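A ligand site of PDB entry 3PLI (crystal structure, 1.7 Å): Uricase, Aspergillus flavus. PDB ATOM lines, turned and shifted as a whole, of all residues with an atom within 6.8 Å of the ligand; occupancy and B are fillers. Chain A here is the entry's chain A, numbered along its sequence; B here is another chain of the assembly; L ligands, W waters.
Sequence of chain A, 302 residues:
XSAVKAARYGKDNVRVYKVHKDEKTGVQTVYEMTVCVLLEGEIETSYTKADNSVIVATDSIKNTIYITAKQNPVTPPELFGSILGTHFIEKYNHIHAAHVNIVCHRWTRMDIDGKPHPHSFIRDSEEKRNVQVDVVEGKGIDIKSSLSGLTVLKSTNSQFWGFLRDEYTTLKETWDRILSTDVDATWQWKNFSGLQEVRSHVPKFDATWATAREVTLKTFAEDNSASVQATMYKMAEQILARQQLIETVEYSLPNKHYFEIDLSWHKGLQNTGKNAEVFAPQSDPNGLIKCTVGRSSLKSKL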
ATOM      1  N   SER A 158      29.889  -2.089 -15.599  1.00  0.00           N
ATOM      2  CA  SER A 158      29.806  -3.230 -16.496  1.00  0.00           C
ATOM      3  C   SER A 158      30.860  -2.984 -17.555  1.00  0.00           C
ATOM      4  O   SER A 158      31.004  -1.861 -18.057  1.00  0.00           O
ATOM      5  CB  SER A 158      28.410  -3.343 -17.136  1.00  0.00           C
ATOM      6  OG  SER A 158      28.419  -4.308 -18.178  1.00  0.00           O
ATOM      7  N   GLN A 159      31.602  -4.034 -17.892  1.00  0.00           N
ATOM      8  CA  GLN A 159      32.678  -3.981 -18.866  1.00  0.00           C
ATOM      9  C   GLN A 159      32.510  -5.133 -19.833  1.00  0.00           C
ATOM     10  O   GLN A 159      31.850  -6.129 -19.536  1.00  0.00           O
ATOM     11  CB  GLN A 159      34.050  -4.134 -18.160  1.00  0.00           C
ATOM     12  CG  GLN A 159      34.224  -3.189 -16.991  1.00  0.00           C
ATOM     13  CD  GLN A 159      35.644  -3.196 -16.398  1.00  0.00           C
ATOM     14  OE1 GLN A 159      36.511  -3.963 -16.824  1.00  0.00           O
ATOM     15  NE2 GLN A 159      35.864  -2.325 -15.425  1.00  0.00           N
ATOM     16  N   PHE A 160      33.138  -5.005 -20.994  1.00  0.00           N
ATOM     17  CA  PHE A 160      33.221  -6.118 -21.914  1.00  0.00           C
ATOM     18  C   PHE A 160      34.399  -5.924 -22.852  1.00  0.00           C
ATOM     19  O   PHE A 160      34.321  -5.185 -23.823  1.00  0.00           O
ATOM     20  CB  PHE A 160      31.868  -6.373 -22.664  1.00  0.00           C
ATOM     21  CG  PHE A 160      31.850  -7.693 -23.384  1.00  0.00           C
ATOM     22  CD1 PHE A 160      31.920  -8.899 -22.669  1.00  0.00           C
ATOM     23  CD2 PHE A 160      31.820  -7.749 -24.789  1.00  0.00           C
ATOM     24  CE1 PHE A 160      31.955 -10.138 -23.343  1.00  0.00           C
ATOM     25  CE2 PHE A 160      31.837  -8.975 -25.461  1.00  0.00           C
ATOM     26  CZ  PHE A 160      31.925 -10.180 -24.730  1.00  0.00           C
ATOM     27  N   PHE A 163      37.381 -10.140 -25.737  1.00  0.00           N
ATOM     28  CA  PHE A 163      36.735 -11.187 -26.513  1.00  0.00           C
ATOM     29  C   PHE A 163      37.475 -11.493 -27.834  1.00  0.00           C
ATOM     30  O   PHE A 163      38.354 -10.731 -28.263  1.00  0.00           O
ATOM     31  CB  PHE A 163      35.248 -10.816 -26.808  1.00  0.00           C
ATOM     32  CG  PHE A 163      35.071  -9.419 -27.312  1.00  0.00           C
ATOM     33  CD1 PHE A 163      34.883  -8.368 -26.429  1.00  0.00           C
ATOM     34  CD2 PHE A 163      35.085  -9.150 -28.698  1.00  0.00           C
ATOM     35  CE1 PHE A 163      34.714  -7.060 -26.876  1.00  0.00           C
ATOM     36  CE2 PHE A 163      34.909  -7.837 -29.156  1.00  0.00           C
ATOM     37  CZ  PHE A 163      34.738  -6.795 -28.242  1.00  0.00           C
ATOM     38  N   LEU A 171      32.749  -4.969 -33.051  1.00  0.00           N
ATOM     39  CA  LEU A 171      32.478  -4.476 -31.704  1.00  0.00           C
ATOM     40  C   LEU A 171      33.733  -3.930 -31.026  1.00  0.00           C
ATOM     41  O   LEU A 171      34.761  -4.630 -30.977  1.00  0.00           O
ATOM     42  CB  LEU A 171      31.896  -5.598 -30.839  1.00  0.00           C
ATOM     43  CG  LEU A 171      31.468  -5.199 -29.408  1.00  0.00           C
ATOM     44  CD1 LEU A 171      30.279  -4.234 -29.404  1.00  0.00           C
ATOM     45  CD2 LEU A 171      31.140  -6.455 -28.596  1.00  0.00           C
ATOM     46  N   ARG A 177      29.933   0.397 -19.618  1.00  0.00           N
ATOM     47  CA  ARG A 177      28.740   0.338 -20.473  1.00  0.00           C
ATOM     48  C   ARG A 177      27.522   0.186 -19.580  1.00  0.00           C
ATOM     49  O   ARG A 177      27.640  -0.109 -18.386  1.00  0.00           O
ATOM     50  CB  ARG A 177      28.799  -0.832 -21.456  1.00  0.00           C
ATOM     51  CG  ARG A 177      28.825  -2.189 -20.758  1.00  0.00           C
ATOM     52  CD  ARG A 177      28.849  -3.336 -21.771  1.00  0.00           C
ATOM     53  NE  ARG A 177      28.659  -4.616 -21.078  1.00  0.00           N
ATOM     54  CZ  ARG A 177      28.461  -5.798 -21.681  1.00  0.00           C
ATOM     55  NH1 ARG A 177      28.462  -5.907 -23.013  1.00  0.00           N
ATOM     56  NH2 ARG A 177      28.299  -6.882 -20.926  1.00  0.00           N
ATOM     57  N   LEU A 179      24.276  -1.979 -18.580  1.00  0.00           N
ATOM     58  CA  LEU A 179      23.865  -3.394 -18.606  1.00  0.00           C
ATOM     59  C   LEU A 179      22.430  -3.489 -18.157  1.00  0.00           C
ATOM     60  O   LEU A 179      22.079  -3.055 -17.061  1.00  0.00           O
ATOM     61  CB  LEU A 179      24.774  -4.238 -17.721  1.00  0.00           C
ATOM     62  CG  LEU A 179      24.460  -5.725 -17.656  1.00  0.00           C
ATOM     63  CD1 LEU A 179      24.610  -6.376 -19.018  1.00  0.00           C
ATOM     64  CD2 LEU A 179      25.417  -6.410 -16.648  1.00  0.00           C
ATOM     65  N   SER A 225      30.952  -6.043 -13.411  1.00  0.00           N
ATOM     66  CA  SER A 225      30.697  -7.169 -14.275  1.00  0.00           C
ATOM     67  C   SER A 225      31.673  -7.269 -15.455  1.00  0.00           C
ATOM     68  O   SER A 225      31.868  -6.319 -16.222  1.00  0.00           O
ATOM     69  CB  SER A 225      29.239  -7.086 -14.761  1.00  0.00           C
ATOM     70  OG  SER A 225      29.015  -8.066 -15.754  1.00  0.00           O
ATOM     71  N   ALA A 226      32.273  -8.437 -15.618  1.00  0.00           N
ATOM     72  CA  ALA A 226      33.197  -8.666 -16.701  1.00  0.00           C
ATOM     73  C   ALA A 226      32.472  -9.107 -17.964  1.00  0.00           C
ATOM     74  O   ALA A 226      33.039  -9.094 -19.061  1.00  0.00           O
ATOM     75  CB  ALA A 226      34.214  -9.740 -16.286  1.00  0.00           C
ATOM     76  N   SER A 227      31.211  -9.540 -17.786  1.00  0.00           N
ATOM     77  CA  SER A 227      30.370 -10.043 -18.888  1.00  0.00           C
ATOM     78  C   SER A 227      29.075 -10.502 -18.237  1.00  0.00           C
ATOM     79  O   SER A 227      29.025 -10.701 -17.025  1.00  0.00           O
ATOM     80  CB  SER A 227      30.987 -11.234 -19.645  1.00  0.00           C
ATOM     81  OG  SER A 227      31.131 -12.389 -18.782  1.00  0.00           O
ATOM     82  N   VAL A 228      28.044 -10.721 -19.057  1.00  0.00           N
ATOM     83  CA  VAL A 228      26.820 -11.273 -18.507  1.00  0.00           C
ATOM     84  C   VAL A 228      27.112 -12.683 -17.967  1.00  0.00           C
ATOM     85  O   VAL A 228      26.619 -13.063 -16.909  1.00  0.00           O
ATOM     86  CB  VAL A 228      25.737 -11.309 -19.606  1.00  0.00           C
ATOM     87  CG1 VAL A 228      24.516 -12.065 -19.136  1.00  0.00           C
ATOM     88  CG2 VAL A 228      25.374  -9.873 -19.950  1.00  0.00           C
ATOM     89  N   GLN A 229      27.907 -13.424 -18.727  1.00  0.00           N
ATOM     90  CA  GLN A 229      28.306 -14.806 -18.378  1.00  0.00           C
ATOM     91  C   GLN A 229      28.889 -14.852 -16.959  1.00  0.00           C
ATOM     92  O   GLN A 229      28.463 -15.675 -16.122  1.00  0.00           O
ATOM     93  CB  GLN A 229      29.338 -15.319 -19.384  1.00  0.00           C
ATOM     94  CG  GLN A 229      28.774 -15.673 -20.784  1.00  0.00           C
ATOM     95  CD  GLN A 229      28.727 -14.506 -21.764  1.00  0.00           C
ATOM     96  OE1 GLN A 229      28.618 -13.329 -21.387  1.00  0.00           O
ATOM     97  NE2 GLN A 229      28.775 -14.846 -23.051  1.00  0.00           N
ATOM     98  N   ASN A 255      20.570  -9.597 -23.266  1.00  0.00           N
ATOM     99  CA  ASN A 255      21.418  -8.448 -23.067  1.00  0.00           C
ATOM    100  C   ASN A 255      20.748  -7.351 -23.892  1.00  0.00           C
ATOM    101  O   ASN A 255      20.822  -7.402 -25.100  1.00  0.00           O
ATOM    102  CB  ASN A 255      22.840  -8.788 -23.554  1.00  0.00           C
ATOM    103  CG  ASN A 255      23.850  -7.694 -23.233  1.00  0.00           C
ATOM    104  OD1 ASN A 255      23.515  -6.692 -22.607  1.00  0.00           O
ATOM    105  ND2 ASN A 255      25.106  -7.895 -23.650  1.00  0.00           N
ATOM    106  N   HIS A 257      20.460  -3.984 -25.364  1.00  0.00           N
ATOM    107  CA  HIS A 257      21.520  -3.014 -25.669  1.00  0.00           C
ATOM    108  C   HIS A 257      21.052  -1.571 -25.670  1.00  0.00           C
ATOM    109  O   HIS A 257      19.965  -1.252 -26.139  1.00  0.00           O
ATOM    110  CB  HIS A 257      22.145  -3.329 -27.020  1.00  0.00           C
ATOM    111  CG  HIS A 257      22.592  -4.746 -27.150  1.00  0.00           C
ATOM    112  ND1 HIS A 257      23.634  -5.255 -26.415  1.00  0.00           N
ATOM    113  CD2 HIS A 257      22.112  -5.777 -27.880  1.00  0.00           C
ATOM    114  CE1 HIS A 257      23.817  -6.532 -26.729  1.00  0.00           C
ATOM    115  NE2 HIS A 257      22.891  -6.875 -27.607  1.00  0.00           N
ATOM    116  N   GLY A 287      21.401  -9.810 -27.340  1.00  0.00           N
ATOM    117  CA  GLY A 287      22.132 -10.976 -26.891  1.00  0.00           C
ATOM    118  C   GLY A 287      21.230 -11.858 -26.040  1.00  0.00           C
ATOM    119  O   GLY A 287      20.261 -11.395 -25.438  1.00  0.00           O
ATOM    120  N   ILE A 289      21.906 -15.084 -23.259  1.00  0.00           N
ATOM    121  CA  ILE A 289      22.993 -15.809 -22.601  1.00  0.00           C
ATOM    122  C   ILE A 289      22.343 -16.754 -21.619  1.00  0.00           C
ATOM    123  O   ILE A 289      21.530 -16.314 -20.816  1.00  0.00           O
ATOM    124  CB  ILE A 289      23.928 -14.834 -21.810  1.00  0.00           C
ATOM    125  CG1 ILE A 289      24.292 -13.573 -22.644  1.00  0.00           C
ATOM    126  CG2 ILE A 289      25.196 -15.603 -21.332  1.00  0.00           C
ATOM    127  CD1 ILE A 289      24.988 -13.823 -23.894  1.00  0.00           C
ATOM    128  N   TYR B   9      24.911 -19.463 -25.798  1.00  0.00           N
ATOM    129  CA  TYR B   9      24.745 -18.012 -25.834  1.00  0.00           C
ATOM    130  C   TYR B   9      24.768 -17.615 -27.305  1.00  0.00           C
ATOM    131  O   TYR B   9      25.266 -18.348 -28.167  1.00  0.00           O
ATOM    132  CB  TYR B   9      25.846 -17.308 -25.009  1.00  0.00           C
ATOM    133  CG  TYR B   9      27.088 -17.166 -25.829  1.00  0.00           C
ATOM    134  CD1 TYR B   9      27.869 -18.278 -26.115  1.00  0.00           C
ATOM    135  CD2 TYR B   9      27.426 -15.951 -26.414  1.00  0.00           C
ATOM    136  CE1 TYR B   9      28.988 -18.171 -26.955  1.00  0.00           C
ATOM    137  CE2 TYR B   9      28.526 -15.826 -27.222  1.00  0.00           C
ATOM    138  CZ  TYR B   9      29.307 -16.947 -27.494  1.00  0.00           C
ATOM    139  OH  TYR B   9      30.389 -16.823 -28.318  1.00  0.00           O
ATOM    140  N   GLY B  10      24.218 -16.443 -27.602  1.00  0.00           N
ATOM    141  CA  GLY B  10      24.221 -15.962 -28.973  1.00  0.00           C
ATOM    142  C   GLY B  10      23.339 -14.732 -29.149  1.00  0.00           C
ATOM    143  O   GLY B  10      23.208 -13.925 -28.263  1.00  0.00           O
ATOM    144  N   LYS B  11      22.771 -14.587 -30.342  1.00  0.00           N
ATOM    145  CA  LYS B  11      22.000 -13.380 -30.673  1.00  0.00           C
ATOM    146  C   LYS B  11      20.595 -13.813 -31.050  1.00  0.00           C
ATOM    147  O   LYS B  11      20.428 -14.762 -31.819  1.00  0.00           O
ATOM    148  CB  LYS B  11      22.653 -12.646 -31.852  1.00  0.00           C
ATOM    149  CG  LYS B  11      22.271 -11.157 -31.935  1.00  0.00           C
ATOM    150  CD  LYS B  11      22.803 -10.403 -30.724  1.00  0.00           C
ATOM    151  CE  LYS B  11      23.412  -9.085 -31.060  1.00  0.00           C
ATOM    152  NZ  LYS B  11      24.146  -8.514 -29.883  1.00  0.00           N
ATOM    153  N   ASN B  52      37.134 -13.915 -21.344  1.00  0.00           N
ATOM    154  CA  ASN B  52      36.371 -13.581 -22.561  1.00  0.00           C
ATOM    155  C   ASN B  52      37.029 -14.041 -23.855  1.00  0.00           C
ATOM    156  O   ASN B  52      36.457 -13.902 -24.926  1.00  0.00           O
ATOM    157  CB  ASN B  52      36.026 -12.077 -22.595  1.00  0.00           C
ATOM    158  CG  ASN B  52      35.039 -11.673 -21.493  1.00  0.00           C
ATOM    159  OD1 ASN B  52      34.307 -12.514 -20.973  1.00  0.00           O
ATOM    160  ND2 ASN B  52      35.029 -10.400 -21.140  1.00  0.00           N
ATOM    161  N   ILE B  55      34.963 -16.178 -26.126  1.00  0.00           N
ATOM    162  CA  ILE B  55      33.674 -15.659 -26.598  1.00  0.00           C
ATOM    163  C   ILE B  55      33.754 -15.036 -27.991  1.00  0.00           C
ATOM    164  O   ILE B  55      34.483 -14.059 -28.204  1.00  0.00           O
ATOM    165  CB  ILE B  55      33.094 -14.612 -25.635  1.00  0.00           C
ATOM    166  CG1 ILE B  55      32.801 -15.226 -24.259  1.00  0.00           C
ATOM    167  CG2 ILE B  55      31.761 -14.030 -26.222  1.00  0.00           C
ATOM    168  CD1 ILE B  55      32.392 -14.167 -23.218  1.00  0.00           C
ATOM    169  N   VAL B  56      32.996 -15.628 -28.917  1.00  0.00           N
ATOM    170  CA  VAL B  56      32.688 -14.991 -30.203  1.00  0.00           C
ATOM    171  C   VAL B  56      31.581 -14.005 -29.819  1.00  0.00           C
ATOM    172  O   VAL B  56      30.524 -14.433 -29.354  1.00  0.00           O
ATOM    173  CB  VAL B  56      32.207 -16.056 -31.226  1.00  0.00           C
ATOM    174  CG1 VAL B  56      31.765 -15.393 -32.548  1.00  0.00           C
ATOM    175  CG2 VAL B  56      33.332 -17.086 -31.506  1.00  0.00           C
ATOM    176  N   ALA B  57      31.820 -12.694 -29.949  1.00  0.00           N
ATOM    177  CA  ALA B  57      30.866 -11.717 -29.411  1.00  0.00           C
ATOM    178  C   ALA B  57      29.517 -11.883 -30.112  1.00  0.00           C
ATOM    179  O   ALA B  57      29.466 -12.235 -31.280  1.00  0.00           O
ATOM    180  CB  ALA B  57      31.385 -10.280 -29.551  1.00  0.00           C
ATOM    181  N   THR B  58      28.420 -11.650 -29.371  1.00  0.00           N
ATOM    182  CA  THR B  58      27.109 -11.838 -29.979  1.00  0.00           C
ATOM    183  C   THR B  58      26.942 -10.841 -31.123  1.00  0.00           C
ATOM    184  O   THR B  58      26.284 -11.148 -32.110  1.00  0.00           O
ATOM    185  CB  THR B  58      25.974 -11.699 -28.961  1.00  0.00           C
ATOM    186  OG1 THR B  58      25.903 -10.359 -28.481  1.00  0.00           O
ATOM    187  CG2 THR B  58      26.192 -12.689 -27.801  1.00  0.00           C
ATOM    188  N   ASP B  59      27.566  -9.663 -30.999  1.00  0.00           N
ATOM    189  CA  ASP B  59      27.560  -8.672 -32.079  1.00  0.00           C
ATOM    190  C   ASP B  59      28.181  -9.242 -33.361  1.00  0.00           C
ATOM    191  O   ASP B  59      27.704  -8.976 -34.454  1.00  0.00           O
ATOM    192  CB  ASP B  59      28.309  -7.404 -31.649  1.00  0.00           C
ATOM    193  CG  ASP B  59      28.136  -6.285 -32.644  1.00  0.00           C
ATOM    194  OD1 ASP B  59      27.042  -5.669 -32.638  1.00  0.00           O
ATOM    195  OD2 ASP B  59      29.074  -6.026 -33.435  1.00  0.00           O
ATOM    196  N   SER B  60      29.258 -10.025 -33.203  1.00  0.00           N
ATOM    197  CA  SER B  60      29.885 -10.708 -34.345  1.00  0.00           C
ATOM    198  C   SER B  60      28.982 -11.776 -34.944  1.00  0.00           C
ATOM    199  O   SER B  60      28.993 -11.998 -36.158  1.00  0.00           O
ATOM    200  CB  SER B  60      31.247 -11.321 -33.919  1.00  0.00           C
ATOM    201  OG  SER B  60      32.015 -10.315 -33.318  1.00  0.00           O
HETATM  202  N1  LIG L   1      28.476 -11.093 -23.294  1.00  0.00           N
HETATM  203  C1  LIG L   1      28.325  -9.801 -22.917  1.00  0.00           C
HETATM  204  O1  LIG L   1      28.231  -9.577 -21.701  1.00  0.00           O
HETATM  205  N2  LIG L   1      28.302  -8.743 -23.796  1.00  0.00           N
HETATM  206  C2  LIG L   1      28.460  -9.017 -25.112  1.00  0.00           C
HETATM  207  C3  LIG L   1      28.627 -10.395 -25.575  1.00  0.00           C
HETATM  208  C4  LIG L   1      28.628 -11.467 -24.567  1.00  0.00           C
HETATM  209  O2  LIG L   1      28.726 -12.647 -24.919  1.00  0.00           O
HETATM  210  N3  LIG L   1      28.756 -10.400 -26.911  1.00  0.00           N
HETATM  211  N4  LIG L   1      28.678  -9.081 -27.300  1.00  0.00           N
HETATM  212  N5  LIG L   1      28.492  -8.250 -26.210  1.00  0.00           N
HETATM  213  O   HOH W   1      27.785  -5.651 -26.354  1.00  0.00           O
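Phe 160 touches the ligand (CE2 to C2, 3.4 Å).
CD2 of Leu 171 touches N4 of the ligand, 3.8 Å away.
CA of Ser 227 touches O1 of the ligand, 3.6 Å away.
CD2 of Tyr 9 of chain B touches O2 of the ligand, 3.9 Å away.
Ile 55 of chain B touches the ligand.
Ala 57 of chain B touches the ligand.
Asp 59 of chain B touches the ligand (N to N4, 3.9 Å).
Hydrophobic or aromatic side chains that line the ligand: Phe 160, Leu 171, Val 228, Tyr 9 of chain B, Ile 55 of chain B and Ala 57 of chain B.
The nearest printed residue that does not touch the ligand is Ile 289 (4.1 Å).
Water W1 bridges a nitrogen (N5) of the ligand (2.7 Å) and the guanidinium group (NH1) of Arg 177 (3.4 Å).
N of Thr 58 of chain B sits at hydrogen-bond distance from N3 of the ligand (2.8 Å).
OG1 of Thr 58 of chain B sits at hydrogen-bond distance from N3 of the ligand (3.3 Å).
An oxygen (O1) of the ligand lies within hydrogen-bond range of the guanidinium group of Arg 177, at 2.8 Å.
The side-chain amide nitrogen (NE2) of Gln 229 is in hydrogen-bond range of an oxygen (O2) of the ligand, 2.9 Å away.
O1 of the ligand is in hydrogen-bond range of N of Val 228 (2.9 Å).
The side-chain amide nitrogen (ND2) of Asn 255 sits close to a nitrogen (N2) of the ligand.
OG1 of Thr 58 of chain B lies within hydrogen-bond range of NZ of Lys 11 of chain B, at 2.9 Å.
The guanidinium group (NE) of Arg 177 sits at hydrogen-bond distance from the side-chain hydroxyl (OG) of Ser 158 (2.9 Å).
The backbone NH (N) of Gln 229 lies close to the side-chain hydroxyl (OG) of Ser 227 (3.4 Å).
NE2 of His 257 sits at hydrogen-bond distance from O of Asn 255, 3.3 Å away.
The backbone NH (N) of Asn 255 is in hydrogen-bond range of the backbone carbonyl oxygen (O) of Gly 287 (2.8 Å).
The backbone carbonyl oxygen (O) of Ser 227 sits at hydrogen-bond distance from the side-chain hydroxyl (OG) of Ser 225 (2.9 Å).
The side-chain hydroxyl (OH) of Tyr 9 of chain B sits at hydrogen-bond distance from the backbone carbonyl oxygen (O) of Val 56 of chain B, 2.6 Å away.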
